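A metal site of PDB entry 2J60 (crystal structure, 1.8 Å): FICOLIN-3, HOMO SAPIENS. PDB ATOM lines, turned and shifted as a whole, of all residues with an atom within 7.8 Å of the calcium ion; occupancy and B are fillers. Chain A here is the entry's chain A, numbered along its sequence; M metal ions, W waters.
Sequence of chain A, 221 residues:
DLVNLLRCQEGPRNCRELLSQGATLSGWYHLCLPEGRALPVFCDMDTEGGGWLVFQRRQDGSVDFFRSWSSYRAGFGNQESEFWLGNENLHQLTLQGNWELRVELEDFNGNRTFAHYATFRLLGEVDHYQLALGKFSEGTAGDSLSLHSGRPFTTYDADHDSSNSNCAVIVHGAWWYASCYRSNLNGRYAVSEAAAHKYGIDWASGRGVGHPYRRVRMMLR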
ATOM      1  N   THR A 154       6.058  -8.943  14.398  1.00  0.00           N
ATOM      2  CA  THR A 154       6.737  -7.735  14.929  1.00  0.00           C
ATOM      3  C   THR A 154       5.887  -6.868  15.849  1.00  0.00           C
ATOM      4  O   THR A 154       4.669  -6.821  15.733  1.00  0.00           O
ATOM      5  CB  THR A 154       7.543  -6.863  13.901  1.00  0.00           C
ATOM      6  OG1 THR A 154       6.921  -5.598  13.661  1.00  0.00           O
ATOM      7  CG2 THR A 154       7.864  -7.601  12.629  1.00  0.00           C
ATOM      8  N   ALA A 158      10.292  -4.690  18.670  1.00  0.00           N
ATOM      9  CA  ALA A 158      10.902  -5.806  17.959  1.00  0.00           C
ATOM     10  C   ALA A 158      10.489  -5.777  16.492  1.00  0.00           C
ATOM     11  O   ALA A 158       9.539  -6.430  16.083  1.00  0.00           O
ATOM     12  CB  ALA A 158      10.486  -7.111  18.597  1.00  0.00           C
ATOM     13  N   ASP A 159      11.230  -5.009  15.687  1.00  0.00           N
ATOM     14  CA  ASP A 159      10.917  -4.845  14.279  1.00  0.00           C
ATOM     15  C   ASP A 159      11.560  -5.939  13.437  1.00  0.00           C
ATOM     16  O   ASP A 159      12.788  -5.997  13.315  1.00  0.00           O
ATOM     17  CB  ASP A 159      11.378  -3.481  13.794  1.00  0.00           C
ATOM     18  CG  ASP A 159      11.030  -3.237  12.345  1.00  0.00           C
ATOM     19  OD1 ASP A 159      10.671  -4.199  11.619  1.00  0.00           O
ATOM     20  OD2 ASP A 159      11.134  -2.078  11.904  1.00  0.00           O
ATOM     21  N   HIS A 160      10.737  -6.800  12.849  1.00  0.00           N
ATOM     22  CA  HIS A 160      11.244  -7.908  12.058  1.00  0.00           C
ATOM     23  C   HIS A 160      10.621  -7.899  10.678  1.00  0.00           C
ATOM     24  O   HIS A 160      10.813  -8.830   9.893  1.00  0.00           O
ATOM     25  CB  HIS A 160      10.958  -9.246  12.745  1.00  0.00           C
ATOM     26  CG  HIS A 160      11.388  -9.298  14.169  1.00  0.00           C
ATOM     27  ND1 HIS A 160      12.707  -9.275  14.558  1.00  0.00           N
ATOM     28  CD2 HIS A 160      10.656  -9.351  15.314  1.00  0.00           C
ATOM     29  CE1 HIS A 160      12.775  -9.329  15.879  1.00  0.00           C
ATOM     30  NE2 HIS A 160      11.545  -9.373  16.362  1.00  0.00           N
ATOM     31  N   ASP A 161       9.879  -6.847  10.373  1.00  0.00           N
ATOM     32  CA  ASP A 161       9.095  -6.855   9.162  1.00  0.00           C
ATOM     33  C   ASP A 161       9.983  -6.583   7.943  1.00  0.00           C
ATOM     34  O   ASP A 161      11.219  -6.601   8.051  1.00  0.00           O
ATOM     35  CB  ASP A 161       7.963  -5.851   9.274  1.00  0.00           C
ATOM     36  CG  ASP A 161       8.462  -4.427   9.419  1.00  0.00           C
ATOM     37  OD1 ASP A 161       9.485  -4.104   8.788  1.00  0.00           O
ATOM     38  OD2 ASP A 161       7.836  -3.632  10.143  1.00  0.00           O
ATOM     39  N   SER A 162       9.352  -6.320   6.805  1.00  0.00           N
ATOM     40  CA  SER A 162      10.091  -6.129   5.559  1.00  0.00           C
ATOM     41  C   SER A 162      10.019  -4.663   5.186  1.00  0.00           C
ATOM     42  O   SER A 162      10.250  -4.305   4.041  1.00  0.00           O
ATOM     43  CB  SER A 162       9.493  -6.986   4.446  1.00  0.00           C
ATOM     44  OG  SER A 162       8.144  -6.638   4.209  1.00  0.00           O
ATOM     45  N   SER A 163       9.693  -3.818   6.154  1.00  0.00           N
ATOM     46  CA  SER A 163       9.601  -2.391   5.905  1.00  0.00           C
ATOM     47  C   SER A 163      10.841  -1.646   6.343  1.00  0.00           C
ATOM     48  O   SER A 163      11.578  -2.100   7.209  1.00  0.00           O
ATOM     49  CB  SER A 163       8.407  -1.797   6.661  1.00  0.00           C
ATOM     50  OG  SER A 163       8.308  -0.410   6.426  1.00  0.00           O
ATOM     51  N   ASN A 164      11.066  -0.479   5.738  1.00  0.00           N
ATOM     52  CA  ASN A 164      12.163   0.402   6.142  1.00  0.00           C
ATOM     53  C   ASN A 164      11.863   1.055   7.486  1.00  0.00           C
ATOM     54  O   ASN A 164      12.756   1.615   8.123  1.00  0.00           O
ATOM     55  CB  ASN A 164      12.405   1.462   5.076  1.00  0.00           C
ATOM     56  CG  ASN A 164      11.121   1.990   4.474  1.00  0.00           C
ATOM     57  OD1 ASN A 164      10.216   1.227   4.128  1.00  0.00           O
ATOM     58  ND2 ASN A 164      11.023   3.318   4.367  1.00  0.00           N
ATOM     59  N   SER A 165      10.616   0.975   7.896  1.00  0.00           N
ATOM     60  CA  SER A 165      10.228   1.460   9.209  1.00  0.00           C
ATOM     61  C   SER A 165       9.692   0.293  10.038  1.00  0.00           C
ATOM     62  O   SER A 165       9.805  -0.887   9.640  1.00  0.00           O
ATOM     63  CB  SER A 165       9.203   2.585   9.075  1.00  0.00           C
ATOM     64  OG  SER A 165       8.382   2.365   7.950  1.00  0.00           O
ATOM     65  N   ASN A 166       9.137   0.632  11.193  1.00  0.00           N
ATOM     66  CA  ASN A 166       8.559  -0.330  12.094  1.00  0.00           C
ATOM     67  C   ASN A 166       7.048  -0.285  11.969  1.00  0.00           C
ATOM     68  O   ASN A 166       6.397   0.640  12.453  1.00  0.00           O
ATOM     69  CB  ASN A 166       9.034  -0.079  13.532  1.00  0.00           C
ATOM     70  CG  ASN A 166       8.390  -1.006  14.524  1.00  0.00           C
ATOM     71  OD1 ASN A 166       7.225  -1.378  14.368  1.00  0.00           O
ATOM     72  ND2 ASN A 166       9.139  -1.391  15.557  1.00  0.00           N
ATOM     73  N   CYS A 167       6.508  -1.298  11.284  1.00  0.00           N
ATOM     74  CA  CYS A 167       5.092  -1.363  10.902  1.00  0.00           C
ATOM     75  C   CYS A 167       4.114  -1.339  12.078  1.00  0.00           C
ATOM     76  O   CYS A 167       3.002  -0.859  11.932  1.00  0.00           O
ATOM     77  CB  CYS A 167       4.827  -2.654  10.126  1.00  0.00           C
ATOM     78  SG  CYS A 167       5.249  -2.571   8.419  1.00  0.00           S
ATOM     79  N   ALA A 168       4.551  -1.913  13.189  1.00  0.00           N
ATOM     80  CA  ALA A 168       3.777  -1.960  14.423  1.00  0.00           C
ATOM     81  C   ALA A 168       3.534  -0.548  14.922  1.00  0.00           C
ATOM     82  O   ALA A 168       2.437  -0.199  15.280  1.00  0.00           O
ATOM     83  CB  ALA A 168       4.513  -2.773  15.462  1.00  0.00           C
ATOM     84  N   ALA A 178       4.312  -7.366   6.964  1.00  0.00           N
ATOM     85  CA  ALA A 178       5.151  -7.316   5.769  1.00  0.00           C
ATOM     86  C   ALA A 178       5.631  -5.863   5.627  1.00  0.00           C
ATOM     87  O   ALA A 178       6.652  -5.480   6.211  1.00  0.00           O
ATOM     88  CB  ALA A 178       4.346  -7.749   4.555  1.00  0.00           C
ATOM     89  N   SER A 179       4.884  -5.082   4.871  1.00  0.00           N
ATOM     90  CA  SER A 179       5.105  -3.651   4.801  1.00  0.00           C
ATOM     91  C   SER A 179       3.898  -2.943   4.224  1.00  0.00           C
ATOM     92  O   SER A 179       4.022  -2.296   3.187  1.00  0.00           O
ATOM     93  CB  SER A 179       6.344  -3.307   3.962  1.00  0.00           C
ATOM     94  OG  SER A 179       6.319  -3.988   2.727  1.00  0.00           O
HETATM   95 CA    CA M   1      11.345  -2.861   9.583  1.00  0.00          CA
HETATM   96  O   HOH W   1      12.614  -4.468   9.160  1.00  0.00           O
HETATM   97  O   HOH W   2      13.354  -1.600   9.719  1.00  0.00           O
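The side-chain carboxylate of Asp 161 lies within hydrogen-bond range of the backbone NH of Cys 167 (2.9 Å). OG of Ser 163 is in hydrogen-bond range of OD1 of Asn 164, at 3.4 Å. The backbone NH of Ser 165 sits close to the side-chain hydroxyl of Ser 163 (3.1 Å). N of Asn 166 lies close to OD2 of Asp 159 (3.4 Å). The backbone carbonyl oxygen of Ala 178 sits at hydrogen-bond distance from the backbone NH of Ser 163 (3.5 Å).
Of the 14 residues printed, 4 come within 4 Å of the calcium ion.
Water W1 is bound to the calcium ion (2.1 Å). OD1 of Asp 161 binds the calcium ion, 2.4 Å away. The calcium ion is bound by water W2 (2.4 Å). The calcium ion is bound by the side-chain carboxylate (OD2) of Asp 159. O of Ser 163 binds the calcium ion. The calcium ion is bound by the backbone carbonyl oxygen (O) of Ser 165 (2.5 Å). The calcium ion is bound by OD1 of Asp 159, 2.5 Å away. The calcium ion has seven donor atoms within binding distance.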
